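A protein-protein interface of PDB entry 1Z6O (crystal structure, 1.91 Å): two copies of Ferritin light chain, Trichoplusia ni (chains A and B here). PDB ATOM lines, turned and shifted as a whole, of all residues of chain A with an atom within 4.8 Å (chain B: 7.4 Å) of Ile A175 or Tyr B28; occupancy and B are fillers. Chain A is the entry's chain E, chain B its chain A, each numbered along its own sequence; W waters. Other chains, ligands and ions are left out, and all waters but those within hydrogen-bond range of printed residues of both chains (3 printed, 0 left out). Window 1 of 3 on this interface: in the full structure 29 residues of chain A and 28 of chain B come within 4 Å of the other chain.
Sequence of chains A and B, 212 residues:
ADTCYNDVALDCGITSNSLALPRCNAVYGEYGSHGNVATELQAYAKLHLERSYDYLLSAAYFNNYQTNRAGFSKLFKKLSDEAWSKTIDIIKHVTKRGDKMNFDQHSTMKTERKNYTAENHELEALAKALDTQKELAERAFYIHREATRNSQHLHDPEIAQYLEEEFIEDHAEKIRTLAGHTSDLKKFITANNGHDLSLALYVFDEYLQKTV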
ATOM      1  N   LEU A 130     -20.861  29.766   6.350  1.00  0.00           N
ATOM      2  CA  LEU A 130     -19.635  29.121   6.814  1.00  0.00           C
ATOM      3  C   LEU A 130     -19.934  28.281   8.064  1.00  0.00           C
ATOM      4  O   LEU A 130     -19.545  27.111   8.133  1.00  0.00           O
ATOM      5  CB  LEU A 130     -18.560  30.173   7.128  1.00  0.00           C
ATOM      6  CG  LEU A 130     -17.234  29.671   7.721  1.00  0.00           C
ATOM      7  CD1 LEU A 130     -16.540  28.712   6.735  1.00  0.00           C
ATOM      8  CD2 LEU A 130     -16.323  30.882   8.015  1.00  0.00           C
ATOM      9  N   GLN A 133     -21.972  25.129   7.244  1.00  0.00           N
ATOM     10  CA  GLN A 133     -21.200  24.107   6.531  1.00  0.00           C
ATOM     11  C   GLN A 133     -20.240  23.428   7.519  1.00  0.00           C
ATOM     12  O   GLN A 133     -20.038  22.218   7.451  1.00  0.00           O
ATOM     13  CB  GLN A 133     -20.442  24.715   5.336  1.00  0.00           C
ATOM     14  CG  GLN A 133     -21.384  25.111   4.171  1.00  0.00           C
ATOM     15  CD  GLN A 133     -21.994  23.897   3.476  1.00  0.00           C
ATOM     16  OE1 GLN A 133     -23.214  23.797   3.286  1.00  0.00           O
ATOM     17  NE2 GLN A 133     -21.145  22.974   3.092  1.00  0.00           N
ATOM     18  N   LYS A 134     -19.658  24.189   8.447  1.00  0.00           N
ATOM     19  CA  LYS A 134     -18.783  23.573   9.450  1.00  0.00           C
ATOM     20  C   LYS A 134     -19.601  22.607  10.313  1.00  0.00           C
ATOM     21  O   LYS A 134     -19.103  21.559  10.726  1.00  0.00           O
ATOM     22  CB  LYS A 134     -18.138  24.627  10.359  1.00  0.00           C
ATOM     23  CG  LYS A 134     -17.022  25.431   9.683  1.00  0.00           C
ATOM     24  CD  LYS A 134     -16.300  26.329  10.707  1.00  0.00           C
ATOM     25  CE  LYS A 134     -15.208  27.156  10.018  1.00  0.00           C
ATOM     26  NZ  LYS A 134     -14.360  27.907  11.000  1.00  0.00           N
ATOM     27  N   ALA A 137     -20.069  19.479   8.402  1.00  0.00           N
ATOM     28  CA  ALA A 137     -18.793  18.765   8.357  1.00  0.00           C
ATOM     29  C   ALA A 137     -18.478  18.080   9.683  1.00  0.00           C
ATOM     30  O   ALA A 137     -18.031  16.933   9.701  1.00  0.00           O
ATOM     31  CB  ALA A 137     -17.655  19.733   7.977  1.00  0.00           C
ATOM     32  N   GLU A 138     -18.701  18.775  10.795  1.00  0.00           N
ATOM     33  CA  GLU A 138     -18.414  18.178  12.094  1.00  0.00           C
ATOM     34  C   GLU A 138     -19.412  17.076  12.430  1.00  0.00           C
ATOM     35  O   GLU A 138     -19.089  16.145  13.171  1.00  0.00           O
ATOM     36  CB  GLU A 138     -18.371  19.264  13.180  1.00  0.00           C
ATOM     37  CG  GLU A 138     -17.131  20.159  12.991  1.00  0.00           C
ATOM     38  CD  GLU A 138     -17.011  21.270  14.013  1.00  0.00           C
ATOM     39  OE1 GLU A 138     -17.997  21.528  14.727  1.00  0.00           O
ATOM     40  OE2 GLU A 138     -15.929  21.898  14.089  1.00  0.00           O
ATOM     41  N   PHE A 141     -18.000  14.094  10.879  1.00  0.00           N
ATOM     42  CA  PHE A 141     -16.883  13.588  11.692  1.00  0.00           C
ATOM     43  C   PHE A 141     -17.437  12.765  12.862  1.00  0.00           C
ATOM     44  O   PHE A 141     -16.897  11.725  13.227  1.00  0.00           O
ATOM     45  CB  PHE A 141     -16.062  14.748  12.277  1.00  0.00           C
ATOM     46  CG  PHE A 141     -15.029  15.331  11.330  1.00  0.00           C
ATOM     47  CD1 PHE A 141     -15.082  15.085   9.955  1.00  0.00           C
ATOM     48  CD2 PHE A 141     -14.005  16.140  11.831  1.00  0.00           C
ATOM     49  CE1 PHE A 141     -14.120  15.643   9.082  1.00  0.00           C
ATOM     50  CE2 PHE A 141     -13.042  16.701  10.975  1.00  0.00           C
ATOM     51  CZ  PHE A 141     -13.104  16.450   9.592  1.00  0.00           C
ATOM     52  N   ILE A 168     -17.130  14.162   3.395  1.00  0.00           N
ATOM     53  CA  ILE A 168     -15.910  14.678   3.988  1.00  0.00           C
ATOM     54  C   ILE A 168     -14.905  15.360   3.059  1.00  0.00           C
ATOM     55  O   ILE A 168     -14.425  16.452   3.370  1.00  0.00           O
ATOM     56  CB  ILE A 168     -15.266  13.543   4.823  1.00  0.00           C
ATOM     57  CG1 ILE A 168     -16.171  13.276   6.040  1.00  0.00           C
ATOM     58  CG2 ILE A 168     -13.841  13.909   5.260  1.00  0.00           C
ATOM     59  CD1 ILE A 168     -15.827  12.001   6.832  1.00  0.00           C
ATOM     60  N   HIS A 171     -16.417  18.772   1.887  1.00  0.00           N
ATOM     61  CA  HIS A 171     -16.649  19.762   2.937  1.00  0.00           C
ATOM     62  C   HIS A 171     -15.442  20.682   3.101  1.00  0.00           C
ATOM     63  O   HIS A 171     -15.600  21.886   3.278  1.00  0.00           O
ATOM     64  CB  HIS A 171     -16.929  19.081   4.289  1.00  0.00           C
ATOM     65  CG  HIS A 171     -18.308  18.508   4.407  1.00  0.00           C
ATOM     66  ND1 HIS A 171     -18.620  17.496   5.291  1.00  0.00           N
ATOM     67  CD2 HIS A 171     -19.463  18.818   3.765  1.00  0.00           C
ATOM     68  CE1 HIS A 171     -19.909  17.206   5.188  1.00  0.00           C
ATOM     69  NE2 HIS A 171     -20.442  17.994   4.269  1.00  0.00           N
ATOM     70  N   ALA A 172     -14.236  20.124   3.054  1.00  0.00           N
ATOM     71  CA  ALA A 172     -13.036  20.942   3.240  1.00  0.00           C
ATOM     72  C   ALA A 172     -12.935  22.038   2.184  1.00  0.00           C
ATOM     73  O   ALA A 172     -12.578  23.169   2.488  1.00  0.00           O
ATOM     74  CB  ALA A 172     -11.776  20.061   3.212  1.00  0.00           C
ATOM     75  N   GLU A 173     -13.260  21.701   0.942  1.00  0.00           N
ATOM     76  CA  GLU A 173     -13.208  22.683  -0.145  1.00  0.00           C
ATOM     77  C   GLU A 173     -14.242  23.790   0.050  1.00  0.00           C
ATOM     78  O   GLU A 173     -13.941  24.976  -0.130  1.00  0.00           O
ATOM     79  CB  GLU A 173     -13.485  22.003  -1.493  1.00  0.00           C
ATOM     80  CG  GLU A 173     -12.445  20.981  -1.925  1.00  0.00           C
ATOM     81  CD  GLU A 173     -11.092  21.611  -2.207  1.00  0.00           C
ATOM     82  OE1 GLU A 173     -11.061  22.752  -2.718  1.00  0.00           O
ATOM     83  OE2 GLU A 173     -10.060  20.959  -1.932  1.00  0.00           O
ATOM     84  N   LYS A 174     -15.470  23.408   0.394  1.00  0.00           N
ATOM     85  CA  LYS A 174     -16.528  24.405   0.583  1.00  0.00           C
ATOM     86  C   LYS A 174     -16.236  25.342   1.740  1.00  0.00           C
ATOM     87  O   LYS A 174     -16.478  26.546   1.653  1.00  0.00           O
ATOM     88  CB  LYS A 174     -17.882  23.737   0.860  1.00  0.00           C
ATOM     89  CG  LYS A 174     -18.586  23.149  -0.347  1.00  0.00           C
ATOM     90  CD  LYS A 174     -19.969  22.641   0.066  1.00  0.00           C
ATOM     91  CE  LYS A 174     -20.763  22.087  -1.110  1.00  0.00           C
ATOM     92  NZ  LYS A 174     -22.123  21.595  -0.700  1.00  0.00           N
ATOM     93  N   ILE A 175     -15.749  24.781   2.842  1.00  0.00           N
ATOM     94  CA  ILE A 175     -15.453  25.582   4.016  1.00  0.00           C
ATOM     95  C   ILE A 175     -14.296  26.533   3.722  1.00  0.00           C
ATOM     96  O   ILE A 175     -14.337  27.700   4.102  1.00  0.00           O
ATOM     97  CB  ILE A 175     -15.154  24.653   5.220  1.00  0.00           C
ATOM     98  CG1 ILE A 175     -16.485  24.032   5.695  1.00  0.00           C
ATOM     99  CG2 ILE A 175     -14.466  25.426   6.356  1.00  0.00           C
ATOM    100  CD1 ILE A 175     -16.317  22.813   6.614  1.00  0.00           C
ATOM    101  N   ARG A 176     -13.273  26.048   3.028  1.00  0.00           N
ATOM    102  CA  ARG A 176     -12.144  26.921   2.699  1.00  0.00           C
ATOM    103  C   ARG A 176     -12.611  28.058   1.781  1.00  0.00           C
ATOM    104  O   ARG A 176     -12.192  29.208   1.929  1.00  0.00           O
ATOM    105  CB  ARG A 176     -11.030  26.118   2.014  1.00  0.00           C
ATOM    106  CG  ARG A 176      -9.895  26.995   1.443  1.00  0.00           C
ATOM    107  CD  ARG A 176      -9.213  27.861   2.529  1.00  0.00           C
ATOM    108  NE  ARG A 176      -8.142  28.666   1.924  1.00  0.00           N
ATOM    109  CZ  ARG A 176      -8.339  29.803   1.264  1.00  0.00           C
ATOM    110  NH1 ARG A 176      -9.571  30.299   1.134  1.00  0.00           N
ATOM    111  NH2 ARG A 176      -7.312  30.417   0.680  1.00  0.00           N
ATOM    112  N   THR A 177     -13.476  27.736   0.827  1.00  0.00           N
ATOM    113  CA  THR A 177     -13.991  28.756  -0.095  1.00  0.00           C
ATOM    114  C   THR A 177     -14.781  29.836   0.652  1.00  0.00           C
ATOM    115  O   THR A 177     -14.554  31.036   0.455  1.00  0.00           O
ATOM    116  CB  THR A 177     -14.896  28.114  -1.169  1.00  0.00           C
ATOM    117  OG1 THR A 177     -14.104  27.227  -1.966  1.00  0.00           O
ATOM    118  CG2 THR A 177     -15.521  29.184  -2.082  1.00  0.00           C
ATOM    119  N   LEU A 178     -15.701  29.410   1.514  1.00  0.00           N
ATOM    120  CA  LEU A 178     -16.506  30.356   2.283  1.00  0.00           C
ATOM    121  C   LEU A 178     -15.656  31.163   3.260  1.00  0.00           C
ATOM    122  O   LEU A 178     -15.896  32.357   3.455  1.00  0.00           O
ATOM    123  CB  LEU A 178     -17.623  29.612   3.036  1.00  0.00           C
ATOM    124  CG  LEU A 178     -18.719  29.051   2.117  1.00  0.00           C
ATOM    125  CD1 LEU A 178     -19.643  28.110   2.904  1.00  0.00           C
ATOM    126  CD2 LEU A 178     -19.529  30.219   1.537  1.00  0.00           C
ATOM    127  N   ALA A 179     -14.662  30.529   3.882  1.00  0.00           N
ATOM    128  CA  ALA A 179     -13.793  31.259   4.810  1.00  0.00           C
ATOM    129  C   ALA A 179     -13.050  32.350   4.027  1.00  0.00           C
ATOM    130  O   ALA A 179     -12.870  33.467   4.519  1.00  0.00           O
ATOM    131  CB  ALA A 179     -12.780  30.310   5.472  1.00  0.00           C
ATOM    132  N   ASN B  25     -12.677  31.454   9.755  1.00  0.00           N
ATOM    133  CA  ASN B  25     -11.513  30.894   9.093  1.00  0.00           C
ATOM    134  C   ASN B  25     -11.956  29.513   8.653  1.00  0.00           C
ATOM    135  O   ASN B  25     -13.120  29.157   8.853  1.00  0.00           O
ATOM    136  CB  ASN B  25     -10.296  30.865  10.039  1.00  0.00           C
ATOM    137  CG  ASN B  25     -10.530  30.061  11.315  1.00  0.00           C
ATOM    138  OD1 ASN B  25      -9.780  30.208  12.279  1.00  0.00           O
ATOM    139  ND2 ASN B  25     -11.532  29.206  11.324  1.00  0.00           N
ATOM    140  N   ALA B  26     -11.059  28.731   8.066  1.00  0.00           N
ATOM    141  CA  ALA B  26     -11.445  27.414   7.571  1.00  0.00           C
ATOM    142  C   ALA B  26     -11.215  26.279   8.568  1.00  0.00           C
ATOM    143  O   ALA B  26     -11.282  25.111   8.200  1.00  0.00           O
ATOM    144  CB  ALA B  26     -10.693  27.124   6.263  1.00  0.00           C
ATOM    145  N   VAL B  27     -10.957  26.614   9.826  1.00  0.00           N
ATOM    146  CA  VAL B  27     -10.706  25.586  10.838  1.00  0.00           C
ATOM    147  C   VAL B  27     -11.993  24.925  11.335  1.00  0.00           C
ATOM    148  O   VAL B  27     -12.941  25.613  11.720  1.00  0.00           O
ATOM    149  CB  VAL B  27      -9.973  26.191  12.074  1.00  0.00           C
ATOM    150  CG1 VAL B  27      -9.814  25.126  13.181  1.00  0.00           C
ATOM    151  CG2 VAL B  27      -8.592  26.738  11.653  1.00  0.00           C
ATOM    152  N   TYR B  28     -12.041  23.596  11.298  1.00  0.00           N
ATOM    153  CA  TYR B  28     -13.199  22.873  11.834  1.00  0.00           C
ATOM    154  C   TYR B  28     -12.697  21.540  12.380  1.00  0.00           C
ATOM    155  O   TYR B  28     -11.557  21.142  12.104  1.00  0.00           O
ATOM    156  CB  TYR B  28     -14.304  22.691  10.774  1.00  0.00           C
ATOM    157  CG  TYR B  28     -13.940  21.835   9.585  1.00  0.00           C
ATOM    158  CD1 TYR B  28     -14.293  20.488   9.538  1.00  0.00           C
ATOM    159  CD2 TYR B  28     -13.257  22.381   8.495  1.00  0.00           C
ATOM    160  CE1 TYR B  28     -13.976  19.696   8.421  1.00  0.00           C
ATOM    161  CE2 TYR B  28     -12.934  21.610   7.382  1.00  0.00           C
ATOM    162  CZ  TYR B  28     -13.297  20.272   7.351  1.00  0.00           C
ATOM    163  OH  TYR B  28     -12.989  19.512   6.247  1.00  0.00           O
ATOM    164  N   GLY B  29     -13.527  20.860  13.167  1.00  0.00           N
ATOM    165  CA  GLY B  29     -13.098  19.608  13.773  1.00  0.00           C
ATOM    166  C   GLY B  29     -11.909  19.881  14.697  1.00  0.00           C
ATOM    167  O   GLY B  29     -11.102  19.000  14.973  1.00  0.00           O
ATOM    168  N   GLU B  30     -11.786  21.109  15.181  1.00  0.00           N
ATOM    169  CA  GLU B  30     -10.640  21.470  16.039  1.00  0.00           C
ATOM    170  C   GLU B  30      -9.269  21.120  15.423  1.00  0.00           C
ATOM    171  O   GLU B  30      -8.314  20.745  16.127  1.00  0.00           O
ATOM    172  CB  GLU B  30     -10.776  20.799  17.406  1.00  0.00           C
ATOM    173  CG  GLU B  30     -11.976  21.303  18.195  1.00  0.00           C
ATOM    174  CD  GLU B  30     -12.102  20.638  19.546  1.00  0.00           C
ATOM    175  OE1 GLU B  30     -12.187  19.391  19.587  1.00  0.00           O
ATOM    176  OE2 GLU B  30     -12.115  21.363  20.565  1.00  0.00           O
ATOM    177  N   TYR B  31      -9.177  21.238  14.103  1.00  0.00           N
ATOM    178  CA  TYR B  31      -7.933  20.946  13.397  1.00  0.00           C
ATOM    179  C   TYR B  31      -6.827  21.829  13.965  1.00  0.00           C
ATOM    180  O   TYR B  31      -6.973  23.048  14.029  1.00  0.00           O
ATOM    181  CB  TYR B  31      -8.096  21.260  11.907  1.00  0.00           C
ATOM    182  CG  TYR B  31      -6.882  20.932  11.082  1.00  0.00           C
ATOM    183  CD1 TYR B  31      -6.622  19.623  10.691  1.00  0.00           C
ATOM    184  CD2 TYR B  31      -5.989  21.928  10.699  1.00  0.00           C
ATOM    185  CE1 TYR B  31      -5.504  19.309   9.938  1.00  0.00           C
ATOM    186  CE2 TYR B  31      -4.857  21.624   9.940  1.00  0.00           C
ATOM    187  CZ  TYR B  31      -4.627  20.308   9.567  1.00  0.00           C
ATOM    188  OH  TYR B  31      -3.512  19.991   8.836  1.00  0.00           O
ATOM    189  N   GLY B  32      -5.721  21.220  14.372  1.00  0.00           N
ATOM    190  CA  GLY B  32      -4.626  22.002  14.914  1.00  0.00           C
ATOM    191  C   GLY B  32      -4.702  22.265  16.416  1.00  0.00           C
ATOM    192  O   GLY B  32      -3.701  22.659  17.010  1.00  0.00           O
ATOM    193  N   HIS B  93      -2.989  21.701   1.053  1.00  0.00           N
ATOM    194  CA  HIS B  93      -3.947  21.049   1.947  1.00  0.00           C
ATOM    195  C   HIS B  93      -3.888  21.662   3.351  1.00  0.00           C
ATOM    196  O   HIS B  93      -4.916  21.852   4.007  1.00  0.00           O
ATOM    197  CB  HIS B  93      -3.680  19.540   2.049  1.00  0.00           C
ATOM    198  CG  HIS B  93      -4.879  18.770   2.505  1.00  0.00           C
ATOM    199  ND1 HIS B  93      -5.839  18.309   1.630  1.00  0.00           N
ATOM    200  CD2 HIS B  93      -5.327  18.466   3.748  1.00  0.00           C
ATOM    201  CE1 HIS B  93      -6.827  17.756   2.313  1.00  0.00           C
ATOM    202  NE2 HIS B  93      -6.542  17.839   3.601  1.00  0.00           N
ATOM    203  N   LYS B  96      -5.743  24.758   3.113  1.00  0.00           N
ATOM    204  CA  LYS B  96      -7.165  24.496   2.880  1.00  0.00           C
ATOM    205  C   LYS B  96      -7.865  24.246   4.224  1.00  0.00           C
ATOM    206  O   LYS B  96      -9.009  24.662   4.427  1.00  0.00           O
ATOM    207  CB  LYS B  96      -7.350  23.258   1.985  1.00  0.00           C
ATOM    208  CG  LYS B  96      -8.824  22.862   1.829  1.00  0.00           C
ATOM    209  CD  LYS B  96      -9.068  21.902   0.658  1.00  0.00           C
ATOM    210  CE  LYS B  96      -8.433  20.555   0.888  1.00  0.00           C
ATOM    211  NZ  LYS B  96      -8.698  19.640  -0.268  1.00  0.00           N
ATOM    212  N   ARG B  97      -7.171  23.570   5.142  1.00  0.00           N
ATOM    213  CA  ARG B  97      -7.736  23.263   6.456  1.00  0.00           C
ATOM    214  C   ARG B  97      -7.576  24.398   7.476  1.00  0.00           C
ATOM    215  O   ARG B  97      -7.792  24.203   8.672  1.00  0.00           O
ATOM    216  CB  ARG B  97      -7.141  21.948   7.003  1.00  0.00           C
ATOM    217  CG  ARG B  97      -7.530  20.691   6.177  1.00  0.00           C
ATOM    218  CD  ARG B  97      -9.062  20.479   6.132  1.00  0.00           C
ATOM    219  NE  ARG B  97      -9.652  20.440   7.470  1.00  0.00           N
ATOM    220  CZ  ARG B  97      -9.656  19.376   8.271  1.00  0.00           C
ATOM    221  NH1 ARG B  97      -9.109  18.227   7.881  1.00  0.00           N
ATOM    222  NH2 ARG B  97     -10.189  19.468   9.483  1.00  0.00           N
ATOM    223  N   GLY B  98      -7.181  25.581   7.004  1.00  0.00           N
ATOM    224  CA  GLY B  98      -7.093  26.734   7.891  1.00  0.00           C
ATOM    225  C   GLY B  98      -5.827  26.934   8.690  1.00  0.00           C
ATOM    226  O   GLY B  98      -5.787  27.754   9.597  1.00  0.00           O
ATOM    227  N   HIS B 155     -10.299  13.423  16.065  1.00  0.00           N
ATOM    228  CA  HIS B 155     -10.759  12.462  15.071  1.00  0.00           C
ATOM    229  C   HIS B 155     -10.905  13.278  13.793  1.00  0.00           C
ATOM    230  O   HIS B 155     -11.834  14.080  13.666  1.00  0.00           O
ATOM    231  CB  HIS B 155     -12.104  11.828  15.435  1.00  0.00           C
ATOM    232  CG  HIS B 155     -12.491  10.712  14.512  1.00  0.00           C
ATOM    233  ND1 HIS B 155     -11.766   9.540  14.424  1.00  0.00           N
ATOM    234  CD2 HIS B 155     -13.484  10.610  13.595  1.00  0.00           C
ATOM    235  CE1 HIS B 155     -12.295   8.766  13.491  1.00  0.00           C
ATOM    236  NE2 HIS B 155     -13.339   9.391  12.970  1.00  0.00           N
ATOM    237  N   ASP B 156      -9.974  13.100  12.857  1.00  0.00           N
ATOM    238  CA  ASP B 156     -10.042  13.861  11.612  1.00  0.00           C
ATOM    239  C   ASP B 156      -9.991  12.937  10.400  1.00  0.00           C
ATOM    240  O   ASP B 156      -8.925  12.648   9.851  1.00  0.00           O
ATOM    241  CB  ASP B 156      -8.914  14.888  11.540  1.00  0.00           C
ATOM    242  CG  ASP B 156      -9.230  15.999  10.560  1.00  0.00           C
ATOM    243  OD1 ASP B 156      -9.484  15.679   9.375  1.00  0.00           O
ATOM    244  OD2 ASP B 156      -9.257  17.180  10.967  1.00  0.00           O
ATOM    245  N   GLU B 158     -10.950  13.584   7.492  1.00  0.00           N
ATOM    246  CA  GLU B 158     -10.667  14.306   6.249  1.00  0.00           C
ATOM    247  C   GLU B 158      -9.179  14.104   5.952  1.00  0.00           C
ATOM    248  O   GLU B 158      -8.799  13.795   4.820  1.00  0.00           O
ATOM    249  CB  GLU B 158     -10.991  15.799   6.388  1.00  0.00           C
ATOM    250  CG  GLU B 158     -11.027  16.552   5.041  1.00  0.00           C
ATOM    251  CD  GLU B 158      -9.642  16.863   4.454  1.00  0.00           C
ATOM    252  OE1 GLU B 158      -9.518  16.841   3.205  1.00  0.00           O
ATOM    253  OE2 GLU B 158      -8.686  17.150   5.218  1.00  0.00           O
ATOM    254  N   ILE B 159      -8.338  14.267   6.968  1.00  0.00           N
ATOM    255  CA  ILE B 159      -6.900  14.039   6.788  1.00  0.00           C
ATOM    256  C   ILE B 159      -6.665  12.555   6.470  1.00  0.00           C
ATOM    257  O   ILE B 159      -5.847  12.213   5.614  1.00  0.00           O
ATOM    258  CB  ILE B 159      -6.094  14.393   8.067  1.00  0.00           C
ATOM    259  CG1 ILE B 159      -6.151  15.904   8.327  1.00  0.00           C
ATOM    260  CG2 ILE B 159      -4.638  13.915   7.917  1.00  0.00           C
ATOM    261  CD1 ILE B 159      -5.620  16.768   7.161  1.00  0.00           C
HETATM  262  O   HOH W   1     -11.301  23.352   5.144  1.00  0.00           O
HETATM  263  O   HOH W   2     -14.248  17.269   5.883  1.00  0.00           O
HETATM  264  O   HOH W   3     -12.585  28.711  13.747  1.00  0.00           O
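Among the printed residues, pairs that only touch across the chains: Ile A168 with Glu B158 (3.3 Å), Ala A179 with Asn B25 (3.4 Å), Arg A176 with Lys B96 (3.5 Å), Ala A179 with Ala B26 (3.5 Å), Phe A141 with His B155 (3.5 Å), Phe A141 with Tyr B28 (3.6 Å), Ile A175 with Tyr B28 (3.6 Å), Glu A138 with Tyr B28 (3.7 Å), Ile A175 with Ala B26 (3.7 Å), Ala A137 with Tyr B28 (3.7 Å), Phe A141 with Asp B156 (3.7 Å), Leu A130 with Asn B25 (3.7 Å), Ala A172 with Lys B96 (3.8 Å), Arg A176 with Ala B26 (3.9 Å), Phe A141 with Glu B158 (3.9 Å) and Ala A172 with Glu B158 (3.9 Å).
No position is printed for both chains.
The backbone carbonyl oxygen of Tyr B28 is in hydrogen-bond range of the guanidinium group of Arg B97 (3.4 Å).
NE2 of His B93 is in hydrogen-bond range of OE2 of Glu B158 (2.8 Å).
OE2 of Glu B158 lies within salt-bridge range of NH1 of Arg B97 (2.9 Å).
OD1 of Asp B156 sits at hydrogen-bond distance from N of Ile B159 (3.0 Å).
OG1 of Thr A177 lies within hydrogen-bond range of O of Glu A173 (2.9 Å).
The side-chain carboxylate of Asp B156 lies close to the backbone NH of Glu B158.
Of the printed residues of chain B, Phe A141 touches Tyr B28, His B155, Asp B156 and Glu B158.
Of the printed residues of chain B, Ala A172 touches Tyr B28, Lys B96 and Glu B158.
Of chain B, only Ala B26 (3.7 Å) and Tyr B28 (3.6 Å) come within 4 Å of Ile A175.
Of the printed residues of chain A, Tyr B28 touches Ala A137 (3.7 Å), Glu A138 (3.7 Å), Phe A141 (3.6 Å), Ala A172 (3.3 Å) and Ile A175 (3.6 Å).
Of the printed residues of chain A, Lys B96 touches Ala A172, Glu A173 and Arg A176.
Arg B97 touches none of the printed residues of chain A.
The side-chain hydroxyl (OH) of Tyr B28 lies close to the backbone NH (N) of Ala A172, at 3.5 Å.
The side-chain amino group (NZ) of Lys B96 is in salt-bridge range of the side-chain carboxylate (OE2) of Glu A173.
O of Asn B25 sits at hydrogen-bond distance from NZ of Lys A134 (2.8 Å).
The side-chain carboxylate (OE2) of Glu A138 sits at hydrogen-bond distance from the backbone NH (N) of Gly B29, 2.8 Å away.
NZ of Lys A134 lies within hydrogen-bond range of O of Val B27, 2.8 Å away.
Water W2 bridges the side-chain hydroxyl (OH) of Tyr B28 (2.6 Å) and the backbone carbonyl oxygen (O) of Ile A168 (2.6 Å).
Water W3 lies within hydrogen-bond range of the side-chain amide nitrogen of Asn B25 (2.7 Å) and the side-chain amino group of Lys A134 (3.4 Å).
Water W1 bridges O of Lys B96 (2.7 Å) and O of Ala A172 (3.0 Å).
Of the 16 printed residues of chain B, 9 touch a printed residue of chain A.
Along chain B the printed residues that touch a printed residue of chain A span positions 25 to 158.
Hydrophobic or aromatic side chains of chain A that line the printed part of chain B: Leu A130, Ala A137, Phe A141, Ile A168, Ala A172, Ile A175 and Ala A179.
Along chain A the printed residues that touch a printed residue of chain B span positions 130 to 179.
Among the printed residues, 21 pairs touch across the chains.
Among the printed residues, Asp or Glu carboxylates within 4 Å of a Lys or Arg side-chain nitrogen of the other chain: Glu A173 with Lys B96 (2.5 Å).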
